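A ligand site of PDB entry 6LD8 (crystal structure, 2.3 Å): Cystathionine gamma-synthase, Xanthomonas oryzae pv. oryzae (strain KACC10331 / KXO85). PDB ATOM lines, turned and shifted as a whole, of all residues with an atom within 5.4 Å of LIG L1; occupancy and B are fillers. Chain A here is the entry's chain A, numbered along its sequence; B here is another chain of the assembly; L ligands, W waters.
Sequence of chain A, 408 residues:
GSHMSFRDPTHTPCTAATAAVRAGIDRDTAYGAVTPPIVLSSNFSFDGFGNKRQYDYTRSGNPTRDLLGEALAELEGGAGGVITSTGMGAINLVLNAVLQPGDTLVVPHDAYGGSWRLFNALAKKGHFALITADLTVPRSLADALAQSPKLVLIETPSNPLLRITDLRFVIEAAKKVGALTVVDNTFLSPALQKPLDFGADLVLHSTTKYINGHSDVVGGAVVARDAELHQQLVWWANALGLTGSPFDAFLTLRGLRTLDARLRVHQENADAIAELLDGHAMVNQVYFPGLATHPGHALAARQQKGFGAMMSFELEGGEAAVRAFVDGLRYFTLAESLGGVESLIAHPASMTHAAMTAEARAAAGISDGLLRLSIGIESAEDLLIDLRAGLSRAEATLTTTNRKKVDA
CB of Thr 86 touches O6 of LIG L1, 3.5 Å away. CD2 of Tyr 112 touches C5 of LIG L1, 3.5 Å away. Glu 155 touches LIG L1 (CD to C8, 3.8 Å). Thr 186 touches LIG L1. Val 218 touches LIG L1 (CG1 to O5, 3.8 Å). O of Gly 219 touches O5 of LIG L1, at 3.6 Å. Leu 338 touches LIG L1. Thr 352 touches LIG L1 (CG2 to O1, 3.1 Å). The nearest printed residue that does not touch LIG L1 is Phe 187 (4.01 Å).
OH of Tyr 57 of chain B sits at hydrogen-bond distance from O7 of LIG L1 (2.5 Å). O of Thr 352 sits close to S1 of LG2 L2 (3.8 Å). The side-chain carboxylate (OD2) of Asp 184 is in hydrogen-bond range of a nitrogen (N2) of LIG L1 (2.6 Å). N1 of LG2 L2 lies within salt-bridge range of OE2 of Glu 336 (3.4 Å). OD1 of Asn 159 sits close to O2 of LIG L1 (2.9 Å). OH of Tyr 112 sits close to S1 of LG2 L2, 2.8 Å away. An oxygen (O6) of LIG L1 sits at hydrogen-bond distance from the backbone NH of Met 88, at 2.7 Å. A nitrogen (N1) of LIG L1 lies close to the side-chain amino group (NZ) of Lys 209 (3.0 Å). O5 of LIG L1 is in hydrogen-bond range of OG1 of Thr 208 (2.8 Å). The guanidinium group (NH1) of Arg 59 of chain B lies within salt-bridge range of an oxygen (O1) of LG2 L2 (2.8 Å). N of Gly 87 sits at hydrogen-bond distance from O5 of LIG L1. OG of Ser 206 sits at hydrogen-bond distance from O5 of LIG L1 (2.8 Å). O1 of LIG L1 is in hydrogen-bond range of N of Ser 337 (2.9 Å). O6 of LIG L1 is in salt-bridge range of NE of Arg 59 of chain B, 2.7 Å away. NH1 of Arg 372 lies within salt-bridge range of O2 of LIG L1 (2.9 Å).
The side-chain hydroxyl of Thr 186 lies within hydrogen-bond range of the side-chain carboxylate of Asp 184. The side-chain hydroxyl of Thr 86 lies within hydrogen-bond range of the backbone NH of Gly 89. The guanidinium group of Arg 372 sits at hydrogen-bond distance from the backbone carbonyl oxygen of Ser 337 (3.1 Å). The backbone NH (N) of Thr 207 is in hydrogen-bond range of the backbone carbonyl oxygen (O) of Gly 219 (2.9 Å). The side-chain hydroxyl (OG1) of Thr 208 sits at hydrogen-bond distance from the backbone NH (N) of Gly 219, 3.0 Å away. The side-chain hydroxyl (OG1) of Thr 186 is in hydrogen-bond range of the backbone NH (N) of Ser 206. NE2 of His 353 sits close to O of Asn 159 (3.3 Å). The guanidinium group (NH2) of Arg 59 of chain B sits at hydrogen-bond distance from the side-chain hydroxyl (OH) of Tyr 112 (3.0 Å).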
ATOM      1  N   THR A  86     -38.035   3.093 -17.928  1.00  0.00           N
ATOM      2  CA  THR A  86     -36.707   3.379 -18.524  1.00  0.00           C
ATOM      3  C   THR A  86     -35.838   2.124 -18.654  1.00  0.00           C
ATOM      4  O   THR A  86     -36.162   1.049 -18.034  1.00  0.00           O
ATOM      5  CB  THR A  86     -35.984   4.449 -17.708  1.00  0.00           C
ATOM      6  OG1 THR A  86     -35.515   3.853 -16.492  1.00  0.00           O
ATOM      7  CG2 THR A  86     -36.860   5.643 -17.393  1.00  0.00           C
ATOM      8  N   GLY A  87     -34.741   2.250 -19.400  1.00  0.00           N
ATOM      9  CA  GLY A  87     -33.736   1.171 -19.491  1.00  0.00           C
ATOM     10  C   GLY A  87     -33.096   0.902 -18.138  1.00  0.00           C
ATOM     11  O   GLY A  87     -33.012  -0.257 -17.726  1.00  0.00           O
ATOM     12  N   MET A  88     -32.702   1.956 -17.422  1.00  0.00           N
ATOM     13  CA  MET A  88     -32.168   1.793 -16.059  1.00  0.00           C
ATOM     14  C   MET A  88     -33.200   1.081 -15.206  1.00  0.00           C
ATOM     15  O   MET A  88     -32.778   0.296 -14.390  1.00  0.00           O
ATOM     16  CB  MET A  88     -31.818   3.114 -15.383  1.00  0.00           C
ATOM     17  CG  MET A  88     -30.547   3.758 -15.880  1.00  0.00           C
ATOM     18  SD  MET A  88     -29.123   2.646 -16.146  1.00  0.00           S
ATOM     19  CE  MET A  88     -29.156   1.772 -14.584  1.00  0.00           C
ATOM     20  N   GLY A  89     -34.487   1.395 -15.355  1.00  0.00           N
ATOM     21  CA  GLY A  89     -35.553   0.713 -14.609  1.00  0.00           C
ATOM     22  C   GLY A  89     -35.599  -0.752 -14.921  1.00  0.00           C
ATOM     23  O   GLY A  89     -35.960  -1.528 -14.049  1.00  0.00           O
ATOM     24  N   ILE A  91     -32.926  -2.601 -15.583  1.00  0.00           N
ATOM     25  CA  ILE A  91     -31.753  -3.096 -14.814  1.00  0.00           C
ATOM     26  C   ILE A  91     -32.170  -3.167 -13.340  1.00  0.00           C
ATOM     27  O   ILE A  91     -32.014  -4.224 -12.684  1.00  0.00           O
ATOM     28  CB  ILE A  91     -30.540  -2.192 -15.065  1.00  0.00           C
ATOM     29  CG1 ILE A  91     -30.113  -2.283 -16.526  1.00  0.00           C
ATOM     30  CG2 ILE A  91     -29.415  -2.501 -14.110  1.00  0.00           C
ATOM     31  CD1 ILE A  91     -28.900  -1.444 -16.852  1.00  0.00           C
ATOM     32  N   TYR A 112     -22.173   0.734 -19.488  1.00  0.00           N
ATOM     33  CA  TYR A 112     -22.749   2.109 -19.524  1.00  0.00           C
ATOM     34  C   TYR A 112     -22.509   2.744 -18.141  1.00  0.00           C
ATOM     35  O   TYR A 112     -22.736   2.051 -17.144  1.00  0.00           O
ATOM     36  CB  TYR A 112     -24.218   2.026 -19.944  1.00  0.00           C
ATOM     37  CG  TYR A 112     -25.021   3.288 -19.724  1.00  0.00           C
ATOM     38  CD1 TYR A 112     -24.587   4.501 -20.240  1.00  0.00           C
ATOM     39  CD2 TYR A 112     -26.173   3.292 -18.936  1.00  0.00           C
ATOM     40  CE1 TYR A 112     -25.256   5.681 -19.996  1.00  0.00           C
ATOM     41  CE2 TYR A 112     -26.876   4.473 -18.708  1.00  0.00           C
ATOM     42  CZ  TYR A 112     -26.415   5.671 -19.224  1.00  0.00           C
ATOM     43  OH  TYR A 112     -27.051   6.857 -19.000  1.00  0.00           O
ATOM     44  N   SER A 115     -25.220   2.423 -15.689  1.00  0.00           N
ATOM     45  CA  SER A 115     -25.215   1.088 -15.063  1.00  0.00           C
ATOM     46  C   SER A 115     -24.258   1.072 -13.861  1.00  0.00           C
ATOM     47  O   SER A 115     -24.611   0.629 -12.751  1.00  0.00           O
ATOM     48  CB  SER A 115     -24.847   0.058 -16.095  1.00  0.00           C
ATOM     49  OG  SER A 115     -25.883  -0.090 -17.064  1.00  0.00           O
ATOM     50  N   GLU A 155     -22.540  -6.897 -20.906  1.00  0.00           N
ATOM     51  CA  GLU A 155     -22.971  -5.847 -21.841  1.00  0.00           C
ATOM     52  C   GLU A 155     -22.086  -5.961 -23.100  1.00  0.00           C
ATOM     53  O   GLU A 155     -20.917  -5.534 -23.044  1.00  0.00           O
ATOM     54  CB  GLU A 155     -22.912  -4.488 -21.129  1.00  0.00           C
ATOM     55  CG  GLU A 155     -23.287  -3.314 -22.036  1.00  0.00           C
ATOM     56  CD  GLU A 155     -22.981  -1.919 -21.489  1.00  0.00           C
ATOM     57  OE1 GLU A 155     -22.329  -1.174 -22.220  1.00  0.00           O
ATOM     58  OE2 GLU A 155     -23.365  -1.609 -20.326  1.00  0.00           O
ATOM     59  N   ASN A 159     -20.356  -0.211 -24.297  1.00  0.00           N
ATOM     60  CA  ASN A 159     -20.557   1.215 -24.538  1.00  0.00           C
ATOM     61  C   ASN A 159     -19.522   1.945 -23.709  1.00  0.00           C
ATOM     62  O   ASN A 159     -19.642   1.933 -22.489  1.00  0.00           O
ATOM     63  CB  ASN A 159     -21.991   1.557 -24.105  1.00  0.00           C
ATOM     64  CG  ASN A 159     -22.340   3.032 -24.151  1.00  0.00           C
ATOM     65  OD1 ASN A 159     -23.430   3.381 -23.674  1.00  0.00           O
ATOM     66  ND2 ASN A 159     -21.448   3.863 -24.697  1.00  0.00           N
ATOM     67  N   ASP A 184     -27.366  -7.203 -21.352  1.00  0.00           N
ATOM     68  CA  ASP A 184     -27.790  -5.900 -21.877  1.00  0.00           C
ATOM     69  C   ASP A 184     -27.498  -5.900 -23.382  1.00  0.00           C
ATOM     70  O   ASP A 184     -26.352  -5.687 -23.771  1.00  0.00           O
ATOM     71  CB  ASP A 184     -27.103  -4.764 -21.122  1.00  0.00           C
ATOM     72  CG  ASP A 184     -27.696  -3.417 -21.506  1.00  0.00           C
ATOM     73  OD1 ASP A 184     -28.373  -3.411 -22.562  1.00  0.00           O
ATOM     74  OD2 ASP A 184     -27.510  -2.408 -20.736  1.00  0.00           O
ATOM     75  N   THR A 186     -28.755  -3.780 -25.684  1.00  0.00           N
ATOM     76  CA  THR A 186     -29.231  -2.475 -26.198  1.00  0.00           C
ATOM     77  C   THR A 186     -28.537  -2.134 -27.533  1.00  0.00           C
ATOM     78  O   THR A 186     -29.207  -1.594 -28.454  1.00  0.00           O
ATOM     79  CB  THR A 186     -28.975  -1.360 -25.168  1.00  0.00           C
ATOM     80  OG1 THR A 186     -29.766  -1.601 -24.004  1.00  0.00           O
ATOM     81  CG2 THR A 186     -29.281   0.028 -25.689  1.00  0.00           C
ATOM     82  N   PHE A 187     -27.216  -2.269 -27.591  1.00  0.00           N
ATOM     83  CA  PHE A 187     -26.385  -1.812 -28.707  1.00  0.00           C
ATOM     84  C   PHE A 187     -26.703  -2.533 -30.028  1.00  0.00           C
ATOM     85  O   PHE A 187     -26.496  -1.891 -31.052  1.00  0.00           O
ATOM     86  CB  PHE A 187     -24.930  -1.889 -28.295  1.00  0.00           C
ATOM     87  CG  PHE A 187     -24.347  -0.571 -27.915  1.00  0.00           C
ATOM     88  CD1 PHE A 187     -25.039   0.293 -27.093  1.00  0.00           C
ATOM     89  CD2 PHE A 187     -23.080  -0.196 -28.354  1.00  0.00           C
ATOM     90  CE1 PHE A 187     -24.494   1.511 -26.726  1.00  0.00           C
ATOM     91  CE2 PHE A 187     -22.553   1.044 -28.030  1.00  0.00           C
ATOM     92  CZ  PHE A 187     -23.261   1.893 -27.218  1.00  0.00           C
ATOM     93  N   SER A 206     -32.517  -1.023 -23.130  1.00  0.00           N
ATOM     94  CA  SER A 206     -33.120   0.316 -23.299  1.00  0.00           C
ATOM     95  C   SER A 206     -33.875   0.396 -24.620  1.00  0.00           C
ATOM     96  O   SER A 206     -33.192   0.490 -25.628  1.00  0.00           O
ATOM     97  CB  SER A 206     -32.072   1.344 -23.223  1.00  0.00           C
ATOM     98  OG  SER A 206     -32.623   2.586 -23.507  1.00  0.00           O
ATOM     99  N   THR A 207     -35.213   0.359 -24.616  1.00  0.00           N
ATOM    100  CA  THR A 207     -36.043   0.538 -25.819  1.00  0.00           C
ATOM    101  C   THR A 207     -35.906   1.962 -26.361  1.00  0.00           C
ATOM    102  O   THR A 207     -36.300   2.214 -27.469  1.00  0.00           O
ATOM    103  CB  THR A 207     -37.525   0.304 -25.541  1.00  0.00           C
ATOM    104  OG1 THR A 207     -37.953   1.223 -24.540  1.00  0.00           O
ATOM    105  CG2 THR A 207     -37.784  -1.129 -25.144  1.00  0.00           C
ATOM    106  N   THR A 208     -35.343   2.858 -25.582  1.00  0.00           N
ATOM    107  CA  THR A 208     -35.048   4.232 -25.956  1.00  0.00           C
ATOM    108  C   THR A 208     -34.235   4.286 -27.249  1.00  0.00           C
ATOM    109  O   THR A 208     -34.222   5.358 -27.933  1.00  0.00           O
ATOM    110  CB  THR A 208     -34.306   4.887 -24.791  1.00  0.00           C
ATOM    111  OG1 THR A 208     -34.997   4.609 -23.571  1.00  0.00           O
ATOM    112  CG2 THR A 208     -34.121   6.370 -24.965  1.00  0.00           C
ATOM    113  N   LYS A 209     -33.465   3.248 -27.540  1.00  0.00           N
ATOM    114  CA  LYS A 209     -32.408   3.315 -28.583  1.00  0.00           C
ATOM    115  C   LYS A 209     -32.994   2.772 -29.889  1.00  0.00           C
ATOM    116  O   LYS A 209     -33.937   3.400 -30.400  1.00  0.00           O
ATOM    117  CB  LYS A 209     -31.177   2.557 -28.100  1.00  0.00           C
ATOM    118  CG  LYS A 209     -30.589   3.041 -26.787  1.00  0.00           C
ATOM    119  CD  LYS A 209     -30.709   4.522 -26.590  1.00  0.00           C
ATOM    120  CE  LYS A 209     -29.965   4.990 -25.354  1.00  0.00           C
ATOM    121  NZ  LYS A 209     -29.557   3.846 -24.520  1.00  0.00           N
ATOM    122  N   VAL A 218     -38.455   7.239 -23.701  1.00  0.00           N
ATOM    123  CA  VAL A 218     -37.527   6.529 -22.810  1.00  0.00           C
ATOM    124  C   VAL A 218     -38.302   5.317 -22.309  1.00  0.00           C
ATOM    125  O   VAL A 218     -39.482   5.490 -21.931  1.00  0.00           O
ATOM    126  CB  VAL A 218     -37.029   7.459 -21.702  1.00  0.00           C
ATOM    127  CG1 VAL A 218     -36.018   6.747 -20.829  1.00  0.00           C
ATOM    128  CG2 VAL A 218     -36.421   8.730 -22.268  1.00  0.00           C
ATOM    129  N   GLY A 219     -37.675   4.138 -22.351  1.00  0.00           N
ATOM    130  CA  GLY A 219     -38.294   2.858 -21.981  1.00  0.00           C
ATOM    131  C   GLY A 219     -37.265   1.743 -21.828  1.00  0.00           C
ATOM    132  O   GLY A 219     -36.134   1.902 -22.315  1.00  0.00           O
ATOM    133  N   GLU A 336     -26.571  13.101 -26.136  1.00  0.00           N
ATOM    134  CA  GLU A 336     -26.565  11.766 -25.511  1.00  0.00           C
ATOM    135  C   GLU A 336     -27.547  10.897 -26.292  1.00  0.00           C
ATOM    136  O   GLU A 336     -28.254  11.435 -27.176  1.00  0.00           O
ATOM    137  CB  GLU A 336     -26.843  11.945 -24.014  1.00  0.00           C
ATOM    138  CG  GLU A 336     -25.590  12.383 -23.252  1.00  0.00           C
ATOM    139  CD  GLU A 336     -25.787  13.039 -21.902  1.00  0.00           C
ATOM    140  OE1 GLU A 336     -24.776  13.425 -21.280  1.00  0.00           O
ATOM    141  OE2 GLU A 336     -26.949  13.190 -21.481  1.00  0.00           O
ATOM    142  N   SER A 337     -27.584   9.614 -25.916  1.00  0.00           N
ATOM    143  CA  SER A 337     -28.426   8.551 -26.498  1.00  0.00           C
ATOM    144  C   SER A 337     -27.826   8.065 -27.838  1.00  0.00           C
ATOM    145  O   SER A 337     -26.710   8.486 -28.241  1.00  0.00           O
ATOM    146  CB  SER A 337     -29.841   9.041 -26.637  1.00  0.00           C
ATOM    147  OG  SER A 337     -30.775   7.960 -26.674  1.00  0.00           O
ATOM    148  N   LEU A 338     -28.562   7.219 -28.538  1.00  0.00           N
ATOM    149  CA  LEU A 338     -28.041   6.450 -29.695  1.00  0.00           C
ATOM    150  C   LEU A 338     -29.204   5.637 -30.214  1.00  0.00           C
ATOM    151  O   LEU A 338     -30.227   5.499 -29.485  1.00  0.00           O
ATOM    152  CB  LEU A 338     -26.907   5.504 -29.286  1.00  0.00           C
ATOM    153  CG  LEU A 338     -27.291   4.492 -28.205  1.00  0.00           C
ATOM    154  CD1 LEU A 338     -27.409   3.088 -28.754  1.00  0.00           C
ATOM    155  CD2 LEU A 338     -26.296   4.533 -27.039  1.00  0.00           C
ATOM    156  N   THR A 352     -21.890  10.807 -21.544  1.00  0.00           N
ATOM    157  CA  THR A 352     -22.559   9.509 -21.242  1.00  0.00           C
ATOM    158  C   THR A 352     -21.881   8.785 -20.065  1.00  0.00           C
ATOM    159  O   THR A 352     -22.522   7.865 -19.461  1.00  0.00           O
ATOM    160  CB  THR A 352     -22.507   8.621 -22.484  1.00  0.00           C
ATOM    161  OG1 THR A 352     -21.136   8.694 -22.890  1.00  0.00           O
ATOM    162  CG2 THR A 352     -23.489   9.076 -23.553  1.00  0.00           C
ATOM    163  N   HIS A 353     -20.595   9.087 -19.812  1.00  0.00           N
ATOM    164  CA  HIS A 353     -19.788   8.320 -18.841  1.00  0.00           C
ATOM    165  C   HIS A 353     -19.309   9.303 -17.771  1.00  0.00           C
ATOM    166  O   HIS A 353     -18.456   8.892 -16.961  1.00  0.00           O
ATOM    167  CB  HIS A 353     -18.721   7.485 -19.603  1.00  0.00           C
ATOM    168  CG  HIS A 353     -19.330   6.352 -20.384  1.00  0.00           C
ATOM    169  ND1 HIS A 353     -19.250   5.026 -19.965  1.00  0.00           N
ATOM    170  CD2 HIS A 353     -20.070   6.342 -21.510  1.00  0.00           C
ATOM    171  CE1 HIS A 353     -19.913   4.244 -20.800  1.00  0.00           C
ATOM    172  NE2 HIS A 353     -20.440   5.032 -21.768  1.00  0.00           N
ATOM    173  N   ARG A 372     -17.769   9.102 -29.845  1.00  0.00           N
ATOM    174  CA  ARG A 372     -18.689   7.991 -30.159  1.00  0.00           C
ATOM    175  C   ARG A 372     -19.692   8.506 -31.208  1.00  0.00           C
ATOM    176  O   ARG A 372     -20.258   9.567 -31.020  1.00  0.00           O
ATOM    177  CB  ARG A 372     -19.413   7.557 -28.879  1.00  0.00           C
ATOM    178  CG  ARG A 372     -20.199   6.274 -29.020  1.00  0.00           C
ATOM    179  CD  ARG A 372     -21.083   6.037 -27.816  1.00  0.00           C
ATOM    180  NE  ARG A 372     -22.139   7.009 -27.720  1.00  0.00           N
ATOM    181  CZ  ARG A 372     -23.039   7.012 -26.749  1.00  0.00           C
ATOM    182  NH1 ARG A 372     -22.934   6.140 -25.759  1.00  0.00           N
ATOM    183  NH2 ARG A 372     -24.054   7.880 -26.751  1.00  0.00           N
ATOM    184  N   TYR B  57     -31.144  14.863 -21.000  1.00  0.00           N
ATOM    185  CA  TYR B  57     -31.693  13.513 -21.195  1.00  0.00           C
ATOM    186  C   TYR B  57     -32.933  13.298 -20.318  1.00  0.00           C
ATOM    187  O   TYR B  57     -32.893  13.544 -19.097  1.00  0.00           O
ATOM    188  CB  TYR B  57     -30.586  12.491 -20.928  1.00  0.00           C
ATOM    189  CG  TYR B  57     -30.994  11.089 -21.314  1.00  0.00           C
ATOM    190  CD1 TYR B  57     -31.127  10.744 -22.656  1.00  0.00           C
ATOM    191  CD2 TYR B  57     -31.313  10.150 -20.359  1.00  0.00           C
ATOM    192  CE1 TYR B  57     -31.545   9.485 -23.039  1.00  0.00           C
ATOM    193  CE2 TYR B  57     -31.698   8.864 -20.713  1.00  0.00           C
ATOM    194  CZ  TYR B  57     -31.809   8.535 -22.074  1.00  0.00           C
ATOM    195  OH  TYR B  57     -32.156   7.282 -22.437  1.00  0.00           O
ATOM    196  N   ARG B  59     -34.704  10.959 -18.958  1.00  0.00           N
ATOM    197  CA  ARG B  59     -34.716  10.122 -17.722  1.00  0.00           C
ATOM    198  C   ARG B  59     -34.306  10.977 -16.526  1.00  0.00           C
ATOM    199  O   ARG B  59     -34.918  10.820 -15.494  1.00  0.00           O
ATOM    200  CB  ARG B  59     -33.845   8.866 -17.828  1.00  0.00           C
ATOM    201  CG  ARG B  59     -33.587   8.208 -16.471  1.00  0.00           C
ATOM    202  CD  ARG B  59     -33.125   6.756 -16.504  1.00  0.00           C
ATOM    203  NE  ARG B  59     -32.124   6.512 -17.528  1.00  0.00           N
ATOM    204  CZ  ARG B  59     -30.876   6.997 -17.523  1.00  0.00           C
ATOM    205  NH1 ARG B  59     -30.472   7.790 -16.528  1.00  0.00           N
ATOM    206  NH2 ARG B  59     -30.039   6.677 -18.486  1.00  0.00           N
HETATM  207  O1  LIG L   1     -26.084   7.580 -24.494  1.00  0.00           O
HETATM  208  C1  LIG L   1     -26.024   6.558 -23.792  1.00  0.00           C
HETATM  209  O2  LIG L   1     -24.984   5.880 -23.680  1.00  0.00           O
HETATM  210  C2  LIG L   1     -27.166   6.193 -22.970  1.00  0.00           C
HETATM  211  C3  LIG L   1     -28.023   7.215 -22.454  1.00  0.00           C
HETATM  212  N1  LIG L   1     -27.331   4.823 -22.711  1.00  0.00           N
HETATM  213  C4  LIG L   1     -28.282   4.228 -22.064  1.00  0.00           C
HETATM  214  C5  LIG L   1     -28.196   2.789 -21.763  1.00  0.00           C
HETATM  215  C6  LIG L   1     -27.234   2.008 -22.448  1.00  0.00           C
HETATM  216  O3  LIG L   1     -26.404   2.563 -23.365  1.00  0.00           O
HETATM  217  C7  LIG L   1     -27.121   0.646 -22.178  1.00  0.00           C
HETATM  218  C8  LIG L   1     -26.099  -0.193 -22.897  1.00  0.00           C
HETATM  219  N2  LIG L   1     -27.897   0.071 -21.256  1.00  0.00           N
HETATM  220  C9  LIG L   1     -28.800   0.807 -20.582  1.00  0.00           C
HETATM  221  C10 LIG L   1     -29.008   2.145 -20.800  1.00  0.00           C
HETATM  222  C11 LIG L   1     -30.023   2.863 -19.965  1.00  0.00           C
HETATM  223  O4  LIG L   1     -31.323   3.047 -20.600  1.00  0.00           O
HETATM  224  P1  LIG L   1     -32.248   4.363 -20.371  1.00  0.00           P
HETATM  225  O5  LIG L   1     -33.411   4.047 -21.302  1.00  0.00           O
HETATM  226  O6  LIG L   1     -32.678   4.276 -18.884  1.00  0.00           O
HETATM  227  O7  LIG L   1     -31.453   5.568 -20.743  1.00  0.00           O
HETATM  228  N1  LG2 L   2     -26.999  12.326 -18.213  1.00  0.00           N
HETATM  229  C1  LG2 L   2     -27.805  11.072 -18.338  1.00  0.00           C
HETATM  230  C2  LG2 L   2     -27.625  10.247 -17.056  1.00  0.00           C
HETATM  231  O1  LG2 L   2     -28.014   9.107 -16.931  1.00  0.00           O
HETATM  232  C3  LG2 L   2     -27.505  10.307 -19.645  1.00  0.00           C
HETATM  233  S1  LG2 L   2     -25.977   9.339 -19.721  1.00  0.00           S
HETATM  234  O2  LG2 L   2     -27.087  10.743 -16.074  1.00  0.00           O
HETATM  235  O   HOH W   1     -23.613  -1.634 -24.673  1.00  0.00           O
